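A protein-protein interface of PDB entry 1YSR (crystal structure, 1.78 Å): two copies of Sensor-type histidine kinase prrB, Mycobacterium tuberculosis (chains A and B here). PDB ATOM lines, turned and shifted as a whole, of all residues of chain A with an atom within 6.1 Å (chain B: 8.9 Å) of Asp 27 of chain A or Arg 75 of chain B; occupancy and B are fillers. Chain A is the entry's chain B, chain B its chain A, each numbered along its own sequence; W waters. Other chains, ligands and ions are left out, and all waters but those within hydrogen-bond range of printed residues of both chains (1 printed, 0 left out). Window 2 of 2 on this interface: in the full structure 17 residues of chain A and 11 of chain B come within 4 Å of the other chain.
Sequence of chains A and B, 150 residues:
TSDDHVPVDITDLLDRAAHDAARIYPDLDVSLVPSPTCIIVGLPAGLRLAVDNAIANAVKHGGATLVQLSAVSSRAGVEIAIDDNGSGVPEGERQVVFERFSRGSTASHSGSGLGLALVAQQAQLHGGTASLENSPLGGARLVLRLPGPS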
ATOM      1  N   ILE A  24     -11.819  25.827 -17.071  1.00  0.00           N
ATOM      2  CA  ILE A  24     -11.758  24.714 -17.979  1.00  0.00           C
ATOM      3  C   ILE A  24     -13.080  24.424 -18.682  1.00  0.00           C
ATOM      4  O   ILE A  24     -13.079  23.957 -19.837  1.00  0.00           O
ATOM      5  CB  ILE A  24     -11.251  23.406 -17.272  1.00  0.00           C
ATOM      6  CG1 ILE A  24      -9.866  23.641 -16.652  1.00  0.00           C
ATOM      7  CG2 ILE A  24     -11.188  22.232 -18.287  1.00  0.00           C
ATOM      8  CD1 ILE A  24      -9.288  22.437 -15.916  1.00  0.00           C
ATOM      9  N   TYR A  25     -14.187  24.623 -17.965  1.00  0.00           N
ATOM     10  CA  TYR A  25     -15.489  24.231 -18.470  1.00  0.00           C
ATOM     11  C   TYR A  25     -16.330  25.482 -18.602  1.00  0.00           C
ATOM     12  O   TYR A  25     -16.855  25.991 -17.614  1.00  0.00           O
ATOM     13  CB  TYR A  25     -16.180  23.209 -17.549  1.00  0.00           C
ATOM     14  CG  TYR A  25     -15.349  21.983 -17.224  1.00  0.00           C
ATOM     15  CD1 TYR A  25     -15.228  20.935 -18.145  1.00  0.00           C
ATOM     16  CD2 TYR A  25     -14.687  21.873 -15.978  1.00  0.00           C
ATOM     17  CE1 TYR A  25     -14.503  19.801 -17.842  1.00  0.00           C
ATOM     18  CE2 TYR A  25     -13.949  20.762 -15.670  1.00  0.00           C
ATOM     19  CZ  TYR A  25     -13.851  19.730 -16.583  1.00  0.00           C
ATOM     20  OH  TYR A  25     -13.091  18.617 -16.258  1.00  0.00           O
ATOM     21  N   PRO A  26     -16.472  25.972 -19.843  1.00  0.00           N
ATOM     22  CA  PRO A  26     -17.129  27.282 -20.013  1.00  0.00           C
ATOM     23  C   PRO A  26     -18.650  27.250 -19.725  1.00  0.00           C
ATOM     24  O   PRO A  26     -19.227  28.263 -19.300  1.00  0.00           O
ATOM     25  CB  PRO A  26     -16.815  27.642 -21.472  1.00  0.00           C
ATOM     26  CG  PRO A  26     -16.674  26.296 -22.170  1.00  0.00           C
ATOM     27  CD  PRO A  26     -16.117  25.333 -21.130  1.00  0.00           C
ATOM     28  N   ASP A  27     -19.281  26.090 -19.940  1.00  0.00           N
ATOM     29  CA  ASP A  27     -20.703  25.898 -19.624  1.00  0.00           C
ATOM     30  C   ASP A  27     -21.015  26.107 -18.132  1.00  0.00           C
ATOM     31  O   ASP A  27     -22.143  26.429 -17.749  1.00  0.00           O
ATOM     32  CB  ASP A  27     -21.157  24.468 -20.038  1.00  0.00           C
ATOM     33  CG  ASP A  27     -20.375  23.318 -19.288  1.00  0.00           C
ATOM     34  OD1 ASP A  27     -21.019  22.613 -18.430  1.00  0.00           O
ATOM     35  OD2 ASP A  27     -19.133  23.121 -19.569  1.00  0.00           O
ATOM     36  N   LEU A  28     -20.008  25.930 -17.296  1.00  0.00           N
ATOM     37  CA  LEU A  28     -20.248  25.343 -16.001  1.00  0.00           C
ATOM     38  C   LEU A  28     -20.404  26.361 -14.905  1.00  0.00           C
ATOM     39  O   LEU A  28     -19.602  27.263 -14.783  1.00  0.00           O
ATOM     40  CB  LEU A  28     -19.093  24.381 -15.662  1.00  0.00           C
ATOM     41  CG  LEU A  28     -19.099  23.718 -14.285  1.00  0.00           C
ATOM     42  CD1 LEU A  28     -20.355  22.896 -14.101  1.00  0.00           C
ATOM     43  CD2 LEU A  28     -17.786  22.824 -14.159  1.00  0.00           C
ATOM     44  N   ASP A  29     -21.441  26.195 -14.098  1.00  0.00           N
ATOM     45  CA  ASP A  29     -21.582  26.934 -12.867  1.00  0.00           C
ATOM     46  C   ASP A  29     -21.053  26.024 -11.763  1.00  0.00           C
ATOM     47  O   ASP A  29     -21.719  25.080 -11.353  1.00  0.00           O
ATOM     48  CB  ASP A  29     -23.058  27.294 -12.622  1.00  0.00           C
ATOM     49  CG  ASP A  29     -23.294  28.057 -11.306  1.00  0.00           C
ATOM     50  OD1 ASP A  29     -22.478  27.979 -10.366  1.00  0.00           O
ATOM     51  OD2 ASP A  29     -24.351  28.740 -11.190  1.00  0.00           O
ATOM     52  N   VAL A  59     -19.402  16.621 -15.763  1.00  0.00           N
ATOM     53  CA  VAL A  59     -19.512  17.405 -16.981  1.00  0.00           C
ATOM     54  C   VAL A  59     -19.416  16.562 -18.239  1.00  0.00           C
ATOM     55  O   VAL A  59     -20.335  16.604 -19.082  1.00  0.00           O
ATOM     56  CB  VAL A  59     -18.429  18.511 -17.033  1.00  0.00           C
ATOM     57  CG1 VAL A  59     -18.409  19.136 -18.409  1.00  0.00           C
ATOM     58  CG2 VAL A  59     -18.667  19.553 -15.912  1.00  0.00           C
ATOM     59  N   LYS A  60     -18.324  15.809 -18.400  1.00  0.00           N
ATOM     60  CA  LYS A  60     -18.107  15.089 -19.663  1.00  0.00           C
ATOM     61  C   LYS A  60     -19.133  13.967 -19.854  1.00  0.00           C
ATOM     62  O   LYS A  60     -19.539  13.659 -20.981  1.00  0.00           O
ATOM     63  CB  LYS A  60     -16.645  14.587 -19.786  1.00  0.00           C
ATOM     64  CG  LYS A  60     -15.592  15.717 -19.491  1.00  0.00           C
ATOM     65  CD  LYS A  60     -14.129  15.262 -19.298  1.00  0.00           C
ATOM     66  CE  LYS A  60     -13.177  16.364 -19.774  1.00  0.00           C
ATOM     67  NZ  LYS A  60     -11.802  16.392 -19.101  1.00  0.00           N
ATOM     68  N   GLY A  63     -23.183  15.482 -18.285  1.00  0.00           N
ATOM     69  CA  GLY A  63     -23.626  16.728 -18.911  1.00  0.00           C
ATOM     70  C   GLY A  63     -24.081  17.807 -17.933  1.00  0.00           C
ATOM     71  O   GLY A  63     -24.923  18.619 -18.256  1.00  0.00           O
ATOM     72  N   ALA A  64     -23.514  17.814 -16.727  1.00  0.00           N
ATOM     73  CA  ALA A  64     -23.796  18.827 -15.722  1.00  0.00           C
ATOM     74  C   ALA A  64     -23.466  20.197 -16.256  1.00  0.00           C
ATOM     75  O   ALA A  64     -22.451  20.360 -16.992  1.00  0.00           O
ATOM     76  CB  ALA A  64     -22.984  18.577 -14.447  1.00  0.00           C
ATOM     77  N   THR A  65     -24.315  21.163 -15.877  1.00  0.00           N
ATOM     78  CA  THR A  65     -24.090  22.578 -16.104  1.00  0.00           C
ATOM     79  C   THR A  65     -23.983  23.298 -14.772  1.00  0.00           C
ATOM     80  O   THR A  65     -23.655  24.486 -14.723  1.00  0.00           O
ATOM     81  CB  THR A  65     -25.260  23.221 -16.909  1.00  0.00           C
ATOM     82  OG1 THR A  65     -26.511  22.769 -16.358  1.00  0.00           O
ATOM     83  CG2 THR A  65     -25.183  22.815 -18.384  1.00  0.00           C
ATOM     84  N   LEU A  66     -24.263  22.564 -13.695  1.00  0.00           N
ATOM     85  CA  LEU A  66     -24.221  23.081 -12.333  1.00  0.00           C
ATOM     86  C   LEU A  66     -23.556  22.029 -11.450  1.00  0.00           C
ATOM     87  O   LEU A  66     -24.017  20.843 -11.428  1.00  0.00           O
ATOM     88  CB  LEU A  66     -25.661  23.305 -11.834  1.00  0.00           C
ATOM     89  CG  LEU A  66     -25.895  23.964 -10.461  1.00  0.00           C
ATOM     90  CD1 LEU A  66     -25.581  23.057  -9.318  1.00  0.00           C
ATOM     91  CD2 LEU A  66     -25.115  25.250 -10.338  1.00  0.00           C
ATOM     92  N   CYS B  38      -2.723  22.270 -11.646  1.00  0.00           N
ATOM     93  CA  CYS B  38      -3.026  21.146 -12.508  1.00  0.00           C
ATOM     94  C   CYS B  38      -2.513  19.846 -11.955  1.00  0.00           C
ATOM     95  O   CYS B  38      -1.311  19.674 -11.779  1.00  0.00           O
ATOM     96  CB  CYS B  38      -2.485  21.318 -13.925  1.00  0.00           C
ATOM     97  SG  CYS B  38      -2.853  19.868 -14.961  1.00  0.00           S
ATOM     98  N   VAL B  72      -0.788  25.420 -18.323  1.00  0.00           N
ATOM     99  CA  VAL B  72      -2.115  25.802 -18.808  1.00  0.00           C
ATOM    100  C   VAL B  72      -2.924  24.500 -18.882  1.00  0.00           C
ATOM    101  O   VAL B  72      -2.521  23.561 -19.584  1.00  0.00           O
ATOM    102  CB  VAL B  72      -1.979  26.438 -20.208  1.00  0.00           C
ATOM    103  CG1 VAL B  72      -3.337  26.588 -20.905  1.00  0.00           C
ATOM    104  CG2 VAL B  72      -1.283  27.799 -20.113  1.00  0.00           C
ATOM    105  N   SER B  73      -4.060  24.465 -18.195  1.00  0.00           N
ATOM    106  CA  SER B  73      -4.948  23.290 -18.119  1.00  0.00           C
ATOM    107  C   SER B  73      -6.105  23.326 -19.092  1.00  0.00           C
ATOM    108  O   SER B  73      -6.701  24.384 -19.326  1.00  0.00           O
ATOM    109  CB  SER B  73      -5.600  23.217 -16.732  1.00  0.00           C
ATOM    110  OG  SER B  73      -4.658  23.369 -15.696  1.00  0.00           O
ATOM    111  N   SER B  74      -6.477  22.155 -19.575  1.00  0.00           N
ATOM    112  CA  SER B  74      -7.630  21.993 -20.469  1.00  0.00           C
ATOM    113  C   SER B  74      -8.252  20.625 -20.230  1.00  0.00           C
ATOM    114  O   SER B  74      -7.747  19.832 -19.416  1.00  0.00           O
ATOM    115  CB  SER B  74      -7.190  22.155 -21.940  1.00  0.00           C
ATOM    116  OG  SER B  74      -6.224  21.187 -22.296  1.00  0.00           O
ATOM    117  N   ARG B  75      -9.358  20.342 -20.918  1.00  0.00           N
ATOM    118  CA  ARG B  75      -9.991  19.049 -20.759  1.00  0.00           C
ATOM    119  C   ARG B  75      -9.002  17.984 -21.202  1.00  0.00           C
ATOM    120  O   ARG B  75      -9.017  16.917 -20.682  1.00  0.00           O
ATOM    121  CB  ARG B  75     -11.291  18.971 -21.573  1.00  0.00           C
ATOM    122  CG  ARG B  75     -12.399  19.961 -21.146  1.00  0.00           C
ATOM    123  CD  ARG B  75     -13.410  20.148 -22.343  1.00  0.00           C
ATOM    124  NE  ARG B  75     -14.655  20.859 -21.995  1.00  0.00           N
ATOM    125  CZ  ARG B  75     -15.859  20.282 -21.923  1.00  0.00           C
ATOM    126  NH1 ARG B  75     -16.002  18.970 -22.162  1.00  0.00           N
ATOM    127  NH2 ARG B  75     -16.925  21.007 -21.590  1.00  0.00           N
ATOM    128  N   ALA B  76      -8.130  18.317 -22.158  1.00  0.00           N
ATOM    129  CA  ALA B  76      -7.160  17.386 -22.772  1.00  0.00           C
ATOM    130  C   ALA B  76      -5.965  17.049 -21.874  1.00  0.00           C
ATOM    131  O   ALA B  76      -5.310  16.015 -22.039  1.00  0.00           O
ATOM    132  CB  ALA B  76      -6.667  17.969 -24.101  1.00  0.00           C
ATOM    133  N   GLY B  77      -5.678  17.936 -20.924  1.00  0.00           N
ATOM    134  CA  GLY B  77      -4.612  17.695 -19.945  1.00  0.00           C
ATOM    135  C   GLY B  77      -3.880  18.988 -19.684  1.00  0.00           C
ATOM    136  O   GLY B  77      -4.511  20.013 -19.434  1.00  0.00           O
ATOM    137  N   VAL B  78      -2.552  18.969 -19.770  1.00  0.00           N
ATOM    138  CA  VAL B  78      -1.812  20.177 -19.465  1.00  0.00           C
ATOM    139  C   VAL B  78      -0.718  20.473 -20.504  1.00  0.00           C
ATOM    140  O   VAL B  78      -0.134  19.566 -21.088  1.00  0.00           O
ATOM    141  CB  VAL B  78      -1.198  20.010 -18.074  1.00  0.00           C
ATOM    142  CG1 VAL B  78      -0.204  18.816 -18.060  1.00  0.00           C
ATOM    143  CG2 VAL B  78      -0.551  21.296 -17.537  1.00  0.00           C
ATOM    144  N   LEU B 146       0.856  17.035 -22.211  1.00  0.00           N
ATOM    145  CA  LEU B 146       0.612  15.807 -21.495  1.00  0.00           C
ATOM    146  C   LEU B 146      -0.868  15.567 -21.236  1.00  0.00           C
ATOM    147  O   LEU B 146      -1.581  16.505 -20.856  1.00  0.00           O
ATOM    148  CB  LEU B 146       1.350  15.785 -20.170  1.00  0.00           C
ATOM    149  CG  LEU B 146       2.838  16.010 -20.200  1.00  0.00           C
ATOM    150  CD1 LEU B 146       3.418  15.929 -18.804  1.00  0.00           C
ATOM    151  CD2 LEU B 146       3.584  15.125 -21.182  1.00  0.00           C
ATOM    152  N   PRO B 147      -1.326  14.314 -21.491  1.00  0.00           N
ATOM    153  CA  PRO B 147      -2.726  14.005 -21.325  1.00  0.00           C
ATOM    154  C   PRO B 147      -3.134  13.960 -19.875  1.00  0.00           C
ATOM    155  O   PRO B 147      -2.364  13.494 -19.010  1.00  0.00           O
ATOM    156  CB  PRO B 147      -2.869  12.629 -21.961  1.00  0.00           C
ATOM    157  CG  PRO B 147      -1.577  12.000 -21.872  1.00  0.00           C
ATOM    158  CD  PRO B 147      -0.586  13.174 -22.070  1.00  0.00           C
ATOM    159  N   GLY B 148      -4.341  14.464 -19.631  1.00  0.00           N
ATOM    160  CA  GLY B 148      -4.896  14.526 -18.295  1.00  0.00           C
ATOM    161  C   GLY B 148      -5.421  13.158 -17.883  1.00  0.00           C
ATOM    162  O   GLY B 148      -5.444  12.213 -18.694  1.00  0.00           O
ATOM    163  N   PRO B 149      -5.793  13.021 -16.594  1.00  0.00           N
ATOM    164  CA  PRO B 149      -6.214  11.764 -15.966  1.00  0.00           C
ATOM    165  C   PRO B 149      -7.709  11.430 -15.994  1.00  0.00           C
ATOM    166  O   PRO B 149      -8.088  10.305 -15.588  1.00  0.00           O
ATOM    167  CB  PRO B 149      -5.740  11.950 -14.515  1.00  0.00           C
ATOM    168  CG  PRO B 149      -5.943  13.434 -14.279  1.00  0.00           C
ATOM    169  CD  PRO B 149      -5.658  14.118 -15.595  1.00  0.00           C
ATOM    170  N   SER B 150      -8.519  12.391 -16.442  1.00  0.00           N
ATOM    171  CA  SER B 150      -9.986  12.282 -16.517  1.00  0.00           C
ATOM    172  C   SER B 150     -10.541  12.131 -17.940  1.00  0.00           C
ATOM    173  O   SER B 150      -9.919  12.564 -18.929  1.00  0.00           O
ATOM    174  CB  SER B 150     -10.616  13.526 -15.871  1.00  0.00           C
ATOM    175  OG  SER B 150     -10.173  13.636 -14.527  1.00  0.00           O
ATOM    176  OXT SER B 150     -11.657  11.592 -18.119  1.00  0.00           O
HETATM  177  O   HOH W   1     -10.598  23.337 -21.521  1.00  0.00           O
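OD2 of Asp 27 of chain A is in salt-bridge range of NH2 of Arg 75 of chain B. The side-chain amino group of Lys 60 of chain A sits at hydrogen-bond distance from the backbone carbonyl oxygen of Arg 75 of chain B, 3.2 Å away.
The side-chain hydroxyl (OG) of Ser 74 of chain B sits close to the backbone NH (N) of Ala 76 of chain B (3.4 Å).
Ile 24 of chain A touches Ser 73 of chain B. Ser 74 of chain B touches Ile 24 of chain A. Arg 75 of chain B touches Ile 24 of chain A. Tyr 25 of chain A touches Arg 75 of chain B. Val 59 of chain A touches Arg 75 of chain B.
Of the printed residues of chain B, Ile 24 of chain A touches Ser 73, Ser 74 and Arg 75. Of the printed residues of chain B, Tyr 25 of chain A touches Arg 75 (3.8 Å). No residue of chain B comes within 4 Å of Pro 26 of chain A. Asp 27 of chain A touches just one residue of chain B: Arg 75 (3.7 Å). Printed residues of chain B within 4 Å of Val 59 of chain A: Arg 75 (3.98 Å). Of the printed residues of chain B, Lys 60 of chain A touches Arg 75 (3.2 Å). Ala 64 of chain A touches none of the printed residues of chain B. Of the printed residues of chain A, Ser 74 of chain B touches Ile 24. Arg 75 of chain B touches just these residues of chain A: Ile 24, Tyr 25, Asp 27, Val 59 and Lys 60. The nearest printed residue of chain B that does not touch Ile 24 of chain A is Ala 76 of chain B (6.3 Å).
Along chain A the printed residues that touch a printed residue of chain B span positions 24 to 60. Of the 13 printed residues of chain B, 3 touch a printed residue of chain A. Along chain B the printed residues that touch a printed residue of chain A span positions 73 to 75. Among the printed residues, Asp or Glu carboxylates within 4 Å of a Lys or Arg side-chain nitrogen of the other chain: Asp 27 of chain A with Arg 75 of chain B (3.7 Å).
No position is printed for both chains. Of the 7 pairs that touch across the chains among the printed residues, none has its exchanged pair printed and touching as well.
Water W1 bridges O of Ile 24 of chain A (3.1 Å) and N of Arg 75 of chain B (3.3 Å).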
